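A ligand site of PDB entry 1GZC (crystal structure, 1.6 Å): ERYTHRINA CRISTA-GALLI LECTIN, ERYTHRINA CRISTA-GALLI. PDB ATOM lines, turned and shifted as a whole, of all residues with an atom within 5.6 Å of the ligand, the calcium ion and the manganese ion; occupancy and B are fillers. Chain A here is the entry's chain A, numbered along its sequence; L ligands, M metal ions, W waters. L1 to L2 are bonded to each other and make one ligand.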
ATOM      1  N   PRO A  85       9.280 -32.410   3.145  1.00  0.00           N
ATOM      2  CA  PRO A  85       9.876 -32.539   1.815  1.00  0.00           C
ATOM      3  C   PRO A  85      10.844 -31.371   1.593  1.00  0.00           C
ATOM      4  O   PRO A  85      11.230 -30.684   2.550  1.00  0.00           O
ATOM      5  CB  PRO A  85       8.652 -32.489   0.907  1.00  0.00           C
ATOM      6  CG  PRO A  85       7.742 -31.490   1.595  1.00  0.00           C
ATOM      7  CD  PRO A  85       7.910 -31.857   3.078  1.00  0.00           C
ATOM      8  N   LEU A  86      11.261 -31.132   0.352  1.00  0.00           N
ATOM      9  CA  LEU A  86      12.175 -30.006   0.096  1.00  0.00           C
ATOM     10  C   LEU A  86      11.408 -28.683   0.321  1.00  0.00           C
ATOM     11  O   LEU A  86      10.209 -28.588   0.051  1.00  0.00           O
ATOM     12  CB  LEU A  86      12.647 -30.041  -1.343  1.00  0.00           C
ATOM     13  CG  LEU A  86      13.544 -31.215  -1.705  1.00  0.00           C
ATOM     14  CD1 LEU A  86      13.935 -31.139  -3.159  1.00  0.00           C
ATOM     15  CD2 LEU A  86      14.773 -31.137  -0.778  1.00  0.00           C
ATOM     16  N   ALA A  88      10.300 -24.597  -0.159  1.00  0.00           N
ATOM     17  CA  ALA A  88       9.883 -23.845  -1.347  1.00  0.00           C
ATOM     18  C   ALA A  88       9.087 -22.640  -0.848  1.00  0.00           C
ATOM     19  O   ALA A  88       8.649 -22.645   0.291  1.00  0.00           O
ATOM     20  CB  ALA A  88       8.952 -24.731  -2.205  1.00  0.00           C
ATOM     21  N   ASP A  89       8.898 -21.591  -1.649  1.00  0.00           N
ATOM     22  CA  ASP A  89       9.406 -21.454  -3.019  1.00  0.00           C
ATOM     23  C   ASP A  89      10.375 -20.262  -3.120  1.00  0.00           C
ATOM     24  O   ASP A  89      11.202 -20.250  -4.010  1.00  0.00           O
ATOM     25  CB  ASP A  89       8.252 -21.222  -3.981  1.00  0.00           C
ATOM     26  CG  ASP A  89       7.726 -22.533  -4.610  1.00  0.00           C
ATOM     27  OD1 ASP A  89       8.470 -23.090  -5.476  1.00  0.00           O
ATOM     28  OD2 ASP A  89       6.595 -22.994  -4.234  1.00  0.00           O
ATOM     29  N   TYR A 106       3.389 -20.543  -5.864  1.00  0.00           N
ATOM     30  CA  TYR A 106       4.423 -21.588  -5.962  1.00  0.00           C
ATOM     31  C   TYR A 106       5.678 -21.023  -6.637  1.00  0.00           C
ATOM     32  O   TYR A 106       6.154 -19.952  -6.235  1.00  0.00           O
ATOM     33  CB  TYR A 106       3.884 -22.838  -6.701  1.00  0.00           C
ATOM     34  CG  TYR A 106       2.591 -23.364  -6.096  1.00  0.00           C
ATOM     35  CD1 TYR A 106       2.389 -23.361  -4.726  1.00  0.00           C
ATOM     36  CD2 TYR A 106       1.557 -23.864  -6.916  1.00  0.00           C
ATOM     37  CE1 TYR A 106       1.182 -23.848  -4.162  1.00  0.00           C
ATOM     38  CE2 TYR A 106       0.358 -24.336  -6.379  1.00  0.00           C
ATOM     39  CZ  TYR A 106       0.184 -24.321  -5.008  1.00  0.00           C
ATOM     40  OH  TYR A 106      -1.021 -24.763  -4.493  1.00  0.00           O
ATOM     41  N   GLY A 107       6.220 -21.719  -7.648  1.00  0.00           N
ATOM     42  CA  GLY A 107       7.438 -21.245  -8.280  1.00  0.00           C
ATOM     43  C   GLY A 107       7.340 -19.934  -9.041  1.00  0.00           C
ATOM     44  O   GLY A 107       8.380 -19.381  -9.455  1.00  0.00           O
ATOM     45  N   GLU A 127      14.932 -12.216  -7.666  1.00  0.00           N
ATOM     46  CA  GLU A 127      14.427 -13.298  -6.807  1.00  0.00           C
ATOM     47  C   GLU A 127      15.474 -13.966  -5.929  1.00  0.00           C
ATOM     48  O   GLU A 127      16.668 -13.954  -6.258  1.00  0.00           O
ATOM     49  CB  GLU A 127      13.817 -14.355  -7.724  1.00  0.00           C
ATOM     50  CG  GLU A 127      14.871 -14.982  -8.685  1.00  0.00           C
ATOM     51  CD  GLU A 127      14.338 -16.229  -9.417  1.00  0.00           C
ATOM     52  OE1 GLU A 127      13.249 -16.138 -10.007  1.00  0.00           O
ATOM     53  OE2 GLU A 127      15.056 -17.283  -9.407  1.00  0.00           O
ATOM     54  N   ASP A 129      15.379 -17.538  -4.696  1.00  0.00           N
ATOM     55  CA  ASP A 129      14.598 -18.740  -5.023  1.00  0.00           C
ATOM     56  C   ASP A 129      15.115 -19.981  -4.329  1.00  0.00           C
ATOM     57  O   ASP A 129      16.296 -20.335  -4.460  1.00  0.00           O
ATOM     58  CB  ASP A 129      14.724 -18.902  -6.544  1.00  0.00           C
ATOM     59  CG  ASP A 129      13.822 -19.987  -7.150  1.00  0.00           C
ATOM     60  OD1 ASP A 129      13.236 -20.757  -6.422  1.00  0.00           O
ATOM     61  OD2 ASP A 129      13.700 -20.022  -8.409  1.00  0.00           O
ATOM     62  N   THR A 130      14.217 -20.654  -3.609  1.00  0.00           N
ATOM     63  CA  THR A 130      14.606 -21.792  -2.812  1.00  0.00           C
ATOM     64  C   THR A 130      14.218 -23.171  -3.328  1.00  0.00           C
ATOM     65  O   THR A 130      14.598 -24.175  -2.690  1.00  0.00           O
ATOM     66  CB  THR A 130      14.022 -21.611  -1.421  1.00  0.00           C
ATOM     67  OG1 THR A 130      12.602 -21.453  -1.568  1.00  0.00           O
ATOM     68  CG2 THR A 130      14.596 -20.305  -0.760  1.00  0.00           C
ATOM     69  N   PHE A 131      13.530 -23.250  -4.461  1.00  0.00           N
ATOM     70  CA  PHE A 131      13.111 -24.542  -4.993  1.00  0.00           C
ATOM     71  C   PHE A 131      13.465 -24.612  -6.460  1.00  0.00           C
ATOM     72  O   PHE A 131      13.134 -23.698  -7.215  1.00  0.00           O
ATOM     73  CB  PHE A 131      11.580 -24.727  -4.799  1.00  0.00           C
ATOM     74  CG  PHE A 131      11.089 -26.071  -5.292  1.00  0.00           C
ATOM     75  CD1 PHE A 131      11.087 -27.193  -4.435  1.00  0.00           C
ATOM     76  CD2 PHE A 131      10.718 -26.214  -6.621  1.00  0.00           C
ATOM     77  CE1 PHE A 131      10.707 -28.469  -4.937  1.00  0.00           C
ATOM     78  CE2 PHE A 131      10.333 -27.461  -7.146  1.00  0.00           C
ATOM     79  CZ  PHE A 131      10.337 -28.590  -6.290  1.00  0.00           C
ATOM     80  N   SER A 132      14.142 -25.701  -6.868  1.00  0.00           N
ATOM     81  CA  SER A 132      14.530 -25.827  -8.270  1.00  0.00           C
ATOM     82  C   SER A 132      13.400 -26.401  -9.157  1.00  0.00           C
ATOM     83  O   SER A 132      13.161 -27.631  -9.189  1.00  0.00           O
ATOM     84  CB  SER A 132      15.790 -26.712  -8.410  1.00  0.00           C
ATOM     85  OG  SER A 132      16.261 -26.633  -9.752  1.00  0.00           O
ATOM     86  N   ASN A 133      12.674 -25.521  -9.840  1.00  0.00           N
ATOM     87  CA  ASN A 133      11.608 -25.869 -10.756  1.00  0.00           C
ATOM     88  C   ASN A 133      12.218 -26.331 -12.122  1.00  0.00           C
ATOM     89  O   ASN A 133      13.448 -26.257 -12.347  1.00  0.00           O
ATOM     90  CB  ASN A 133      10.703 -24.638 -10.983  1.00  0.00           C
ATOM     91  CG  ASN A 133       9.980 -24.236  -9.745  1.00  0.00           C
ATOM     92  OD1 ASN A 133      10.431 -23.365  -8.971  1.00  0.00           O
ATOM     93  ND2 ASN A 133       8.843 -24.892  -9.504  1.00  0.00           N
ATOM     94  N   TRP A 135      12.322 -24.934 -14.928  1.00  0.00           N
ATOM     95  CA  TRP A 135      13.021 -23.853 -15.613  1.00  0.00           C
ATOM     96  C   TRP A 135      14.215 -23.269 -14.844  1.00  0.00           C
ATOM     97  O   TRP A 135      14.842 -22.348 -15.311  1.00  0.00           O
ATOM     98  CB  TRP A 135      12.032 -22.696 -15.863  1.00  0.00           C
ATOM     99  CG  TRP A 135      11.393 -22.205 -14.555  1.00  0.00           C
ATOM    100  CD1 TRP A 135      11.949 -21.333 -13.622  1.00  0.00           C
ATOM    101  CD2 TRP A 135      10.119 -22.607 -14.019  1.00  0.00           C
ATOM    102  NE1 TRP A 135      11.084 -21.194 -12.545  1.00  0.00           N
ATOM    103  CE2 TRP A 135       9.961 -21.949 -12.761  1.00  0.00           C
ATOM    104  CE3 TRP A 135       9.099 -23.452 -14.471  1.00  0.00           C
ATOM    105  CZ2 TRP A 135       8.821 -22.122 -11.976  1.00  0.00           C
ATOM    106  CZ3 TRP A 135       7.972 -23.629 -13.681  1.00  0.00           C
ATOM    107  CH2 TRP A 135       7.840 -22.955 -12.436  1.00  0.00           C
ATOM    108  N   ASP A 136      14.525 -23.817 -13.693  1.00  0.00           N
ATOM    109  CA  ASP A 136      15.589 -23.274 -12.822  1.00  0.00           C
ATOM    110  C   ASP A 136      16.921 -24.004 -12.912  1.00  0.00           C
ATOM    111  O   ASP A 136      16.974 -25.147 -13.359  1.00  0.00           O
ATOM    112  CB  ASP A 136      15.182 -23.471 -11.342  1.00  0.00           C
ATOM    113  CG  ASP A 136      14.254 -22.390 -10.808  1.00  0.00           C
ATOM    114  OD1 ASP A 136      14.481 -21.223 -11.152  1.00  0.00           O
ATOM    115  OD2 ASP A 136      13.335 -22.716 -10.029  1.00  0.00           O
ATOM    116  N   PRO A 137      18.008 -23.335 -12.458  1.00  0.00           N
ATOM    117  CA  PRO A 137      19.317 -23.994 -12.430  1.00  0.00           C
ATOM    118  C   PRO A 137      19.108 -24.931 -11.222  1.00  0.00           C
ATOM    119  O   PRO A 137      18.184 -24.742 -10.427  1.00  0.00           O
ATOM    120  CB  PRO A 137      20.285 -22.837 -12.104  1.00  0.00           C
ATOM    121  CG  PRO A 137      19.359 -21.821 -11.331  1.00  0.00           C
ATOM    122  CD  PRO A 137      18.102 -21.891 -12.176  1.00  0.00           C
ATOM    123  N   HIS A 142      19.179 -19.666  -4.954  1.00  0.00           N
ATOM    124  CA  HIS A 142      19.915 -18.860  -5.902  1.00  0.00           C
ATOM    125  C   HIS A 142      19.299 -17.464  -6.020  1.00  0.00           C
ATOM    126  O   HIS A 142      18.098 -17.282  -5.852  1.00  0.00           O
ATOM    127  CB  HIS A 142      19.991 -19.491  -7.337  1.00  0.00           C
ATOM    128  CG  HIS A 142      18.660 -19.864  -7.964  1.00  0.00           C
ATOM    129  ND1 HIS A 142      18.122 -21.137  -7.911  1.00  0.00           N
ATOM    130  CD2 HIS A 142      17.789 -19.115  -8.679  1.00  0.00           C
ATOM    131  CE1 HIS A 142      16.964 -21.151  -8.562  1.00  0.00           C
ATOM    132  NE2 HIS A 142      16.735 -19.935  -9.036  1.00  0.00           N
ATOM    133  N   ILE A 150       9.931 -15.718 -15.359  1.00  0.00           N
ATOM    134  CA  ILE A 150      10.398 -16.401 -14.146  1.00  0.00           C
ATOM    135  C   ILE A 150      11.705 -17.193 -14.508  1.00  0.00           C
ATOM    136  O   ILE A 150      12.410 -17.644 -13.603  1.00  0.00           O
ATOM    137  CB  ILE A 150       9.302 -17.369 -13.611  1.00  0.00           C
ATOM    138  CG1 ILE A 150       9.658 -17.894 -12.226  1.00  0.00           C
ATOM    139  CG2 ILE A 150       9.224 -18.630 -14.545  1.00  0.00           C
ATOM    140  CD1 ILE A 150       9.728 -16.771 -11.133  1.00  0.00           C
ATOM    141  N   SER A 152      15.111 -16.907 -15.171  1.00  0.00           N
ATOM    142  CA  SER A 152      16.101 -15.831 -15.037  1.00  0.00           C
ATOM    143  C   SER A 152      17.101 -15.754 -16.165  1.00  0.00           C
ATOM    144  O   SER A 152      17.568 -16.784 -16.655  1.00  0.00           O
ATOM    145  CB  SER A 152      16.927 -16.004 -13.750  1.00  0.00           C
ATOM    146  OG  SER A 152      16.110 -16.248 -12.605  1.00  0.00           O
ATOM    147  N   THR A 155      21.677 -16.180 -12.933  1.00  0.00           N
ATOM    148  CA  THR A 155      21.524 -16.576 -11.542  1.00  0.00           C
ATOM    149  C   THR A 155      22.871 -16.719 -10.843  1.00  0.00           C
ATOM    150  O   THR A 155      23.928 -16.851 -11.483  1.00  0.00           O
ATOM    151  CB  THR A 155      20.783 -17.914 -11.401  1.00  0.00           C
ATOM    152  OG1 THR A 155      21.513 -18.969 -12.103  1.00  0.00           O
ATOM    153  CG2 THR A 155      19.407 -17.783 -12.006  1.00  0.00           C
ATOM    154  N   THR A 216       5.057 -20.013  -0.533  1.00  0.00           N
ATOM    155  CA  THR A 216       5.436 -21.368  -0.057  1.00  0.00           C
ATOM    156  C   THR A 216       4.827 -22.374  -1.050  1.00  0.00           C
ATOM    157  O   THR A 216       4.081 -21.997  -1.931  1.00  0.00           O
ATOM    158  CB  THR A 216       5.008 -21.674   1.381  1.00  0.00           C
ATOM    159  OG1 THR A 216       3.614 -21.416   1.528  1.00  0.00           O
ATOM    160  CG2 THR A 216       5.805 -20.769   2.318  1.00  0.00           C
ATOM    161  N   GLY A 217       5.193 -23.646  -0.866  1.00  0.00           N
ATOM    162  CA  GLY A 217       4.900 -24.656  -1.869  1.00  0.00           C
ATOM    163  C   GLY A 217       3.595 -25.348  -2.029  1.00  0.00           C
ATOM    164  O   GLY A 217       2.681 -25.116  -1.248  1.00  0.00           O
ATOM    165  N   ALA A 218       3.563 -26.232  -3.032  1.00  0.00           N
ATOM    166  CA  ALA A 218       2.343 -26.940  -3.448  1.00  0.00           C
ATOM    167  C   ALA A 218       2.020 -28.268  -2.762  1.00  0.00           C
ATOM    168  O   ALA A 218       1.075 -28.945  -3.199  1.00  0.00           O
ATOM    169  CB  ALA A 218       2.337 -27.116  -4.969  1.00  0.00           C
ATOM    170  N   GLN A 219       2.773 -28.650  -1.738  1.00  0.00           N
ATOM    171  CA  GLN A 219       2.459 -29.869  -1.001  1.00  0.00           C
ATOM    172  C   GLN A 219       2.797 -29.667   0.459  1.00  0.00           C
ATOM    173  O   GLN A 219       3.613 -28.816   0.796  1.00  0.00           O
ATOM    174  CB  GLN A 219       3.214 -31.094  -1.567  1.00  0.00           C
ATOM    175  CG  GLN A 219       4.715 -31.049  -1.412  1.00  0.00           C
ATOM    176  CD  GLN A 219       5.376 -32.353  -1.871  1.00  0.00           C
ATOM    177  OE1 GLN A 219       5.630 -33.244  -1.056  1.00  0.00           O
ATOM    178  NE2 GLN A 219       5.650 -32.466  -3.154  1.00  0.00           N
ATOM    179  N   ALA A 222       6.166 -28.254   2.281  1.00  0.00           N
ATOM    180  CA  ALA A 222       7.173 -27.716   1.300  1.00  0.00           C
ATOM    181  C   ALA A 222       6.995 -26.201   1.610  1.00  0.00           C
ATOM    182  O   ALA A 222       6.277 -25.460   0.891  1.00  0.00           O
ATOM    183  CB  ALA A 222       6.756 -28.018  -0.175  1.00  0.00           C
HETATM  184  C1  LIG L   1       3.239 -32.182  -6.260  1.00  0.00           C
HETATM  185  C2  LIG L   1       3.465 -30.649  -6.142  1.00  0.00           C
HETATM  186  C3  LIG L   1       4.225 -30.124  -7.368  1.00  0.00           C
HETATM  187  C4  LIG L   1       3.514 -30.499  -8.685  1.00  0.00           C
HETATM  188  C5  LIG L   1       4.369 -30.139  -9.910  1.00  0.00           C
HETATM  189  C6  LIG L   1       2.494 -32.438  -7.564  1.00  0.00           C
HETATM  190  O1  LIG L   1       2.278 -33.812  -7.707  1.00  0.00           O
HETATM  191  O2  LIG L   1       2.501 -32.604  -5.122  1.00  0.00           O
HETATM  192  O3  LIG L   1       4.164 -30.384  -4.927  1.00  0.00           O
HETATM  193  O4  LIG L   1       4.331 -28.644  -7.376  1.00  0.00           O
HETATM  194  O5  LIG L   1       3.318 -31.966  -8.683  1.00  0.00           O
HETATM  195  O6  LIG L   1       3.667 -30.423 -11.114  1.00  0.00           O
HETATM  196  C1  LG2 L   2       5.593 -28.072  -6.984  1.00  0.00           C
HETATM  197  C2  LG2 L   2       5.626 -26.590  -7.348  1.00  0.00           C
HETATM  198  C3  LG2 L   2       7.017 -26.024  -6.851  1.00  0.00           C
HETATM  199  C4  LG2 L   2       7.127 -26.270  -5.339  1.00  0.00           C
HETATM  200  C5  LG2 L   2       6.994 -27.770  -5.051  1.00  0.00           C
HETATM  201  C6  LG2 L   2       7.013 -28.084  -3.561  1.00  0.00           C
HETATM  202  O1  LG2 L   2       5.476 -26.396  -8.767  1.00  0.00           O
HETATM  203  O2  LG2 L   2       7.107 -24.640  -7.175  1.00  0.00           O
HETATM  204  O3  LG2 L   2       6.087 -25.638  -4.602  1.00  0.00           O
HETATM  205  O4  LG2 L   2       5.739 -28.270  -5.573  1.00  0.00           O
HETATM  206  O5  LG2 L   2       7.189 -29.499  -3.422  1.00  0.00           O
HETATM  207 CA    CA M   1      12.058 -21.853  -8.248  1.00  0.00          CA
HETATM  208 MN    MN M   2      14.805 -19.323 -10.130  1.00  0.00          MN
HETATM  209  O   HOH W   1       7.238 -27.171 -10.658  1.00  0.00           O
HETATM  210  O   HOH W   2       8.889 -30.113  -1.798  1.00  0.00           O
HETATM  211  O   HOH W   3      10.512 -21.655  -6.437  1.00  0.00           O
HETATM  212  O   HOH W   4       2.868 -26.636  -9.412  1.00  0.00           O
HETATM  213  O   HOH W   5       7.984 -31.290  -5.530  1.00  0.00           O
HETATM  214  O   HOH W   6      15.931 -18.821 -11.938  1.00  0.00           O
HETATM  215  O   HOH W   7      10.920 -20.193  -9.592  1.00  0.00           O
HETATM  216  O   HOH W   8       5.523 -23.620  -9.650  1.00  0.00           O
HETATM  217  O   HOH W   9      12.855 -18.570 -10.940  1.00  0.00           O
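An oxygen (O2) of LG2 L2 lies within hydrogen-bond range of the side-chain amide nitrogen (ND2) of Asn 133 (2.9 Å). An oxygen (O2) of LG2 L2 lies within hydrogen-bond range of the side-chain carboxylate of Asp 89, 2.7 Å away. The backbone NH of Ala 218 is in hydrogen-bond range of an oxygen (O3) of LG2 L2 (3.0 Å). N of Gly 107 lies within hydrogen-bond range of O2 of LG2 L2 (3.1 Å). NE2 of Gln 219 lies within hydrogen-bond range of O3 of LIG L1, at 3.1 Å.
The side-chain carboxylate (OD1) of Asp 89 lies within hydrogen-bond range of the backbone NH (N) of Gly 107. O of Asp 89 lies close to OG1 of Thr 130. The backbone NH (N) of Gly 217 sits at hydrogen-bond distance from the backbone carbonyl oxygen (O) of Ala 222.
Merely in contact with the ligand: Ala 88 (3.8 Å), Tyr 106 (3.7 Å), Gly 217 (3.1 Å) and Ala 222 (3.4 Å). Hydrophobic or aromatic side chains that line the ligand: Ala 88, Tyr 106, Phe 131, Ala 218 and Ala 222.
Of the 24 residues printed, 4 come within 4 Å of the calcium ion. The nearest printed residue that does not touch the calcium ion is Trp 135 (4.5 Å).
Within 4 Å of the manganese ion: Glu 127, Asp 129, Asp 136 and His 142.
OD1 of Asn 133 is bound to the calcium ion (2.3 Å). OD2 of Asp 136 is bound to the calcium ion (2.4 Å). O of Phe 131 is bound to the calcium ion (2.4 Å). Water W3 is bound to the calcium ion, at 2.4 Å. The calcium ion is bound by water W7 (2.4 Å). OD1 of Asp 129 binds the calcium ion (2.4 Å). The side-chain carboxylate (OD2) of Asp 129 is bound to the calcium ion, at 2.5 Å. The calcium ion has seven donor atoms within binding distance.
The manganese ion is bound by the side-chain carboxylate (OD2) of Asp 129 (2.2 Å), the side-chain carboxylate (OE2) of Glu 127 (2.2 Å), the side-chain carboxylate (OD1) of Asp 136 (2.2 Å), water W6 (2.2 Å), water W9 (2.2 Å) and a ring nitrogen (NE2) of His 142 (2.3 Å). The manganese ion has six donor atoms within binding distance.
Water W7 bridges the backbone carbonyl oxygen (O) of Gly 107 and the indole nitrogen (NE1) of Trp 135. Water W9 lies within hydrogen-bond range of the side-chain carboxylate of Glu 127 (2.6 Å) and the backbone carbonyl oxygen of Ile 150 (2.9 Å). Water W2 lies within hydrogen-bond range of O5 of LG2 L2 and O of Leu 86. Water W1 bridges an oxygen (O1) of LG2 L2 (2.7 Å) and the side-chain amide nitrogen of Asn 133 (3.0 Å). Water W8 lies within hydrogen-bond range of the backbone NH of Gly 107 and an oxygen (O1) of LG2 L2.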
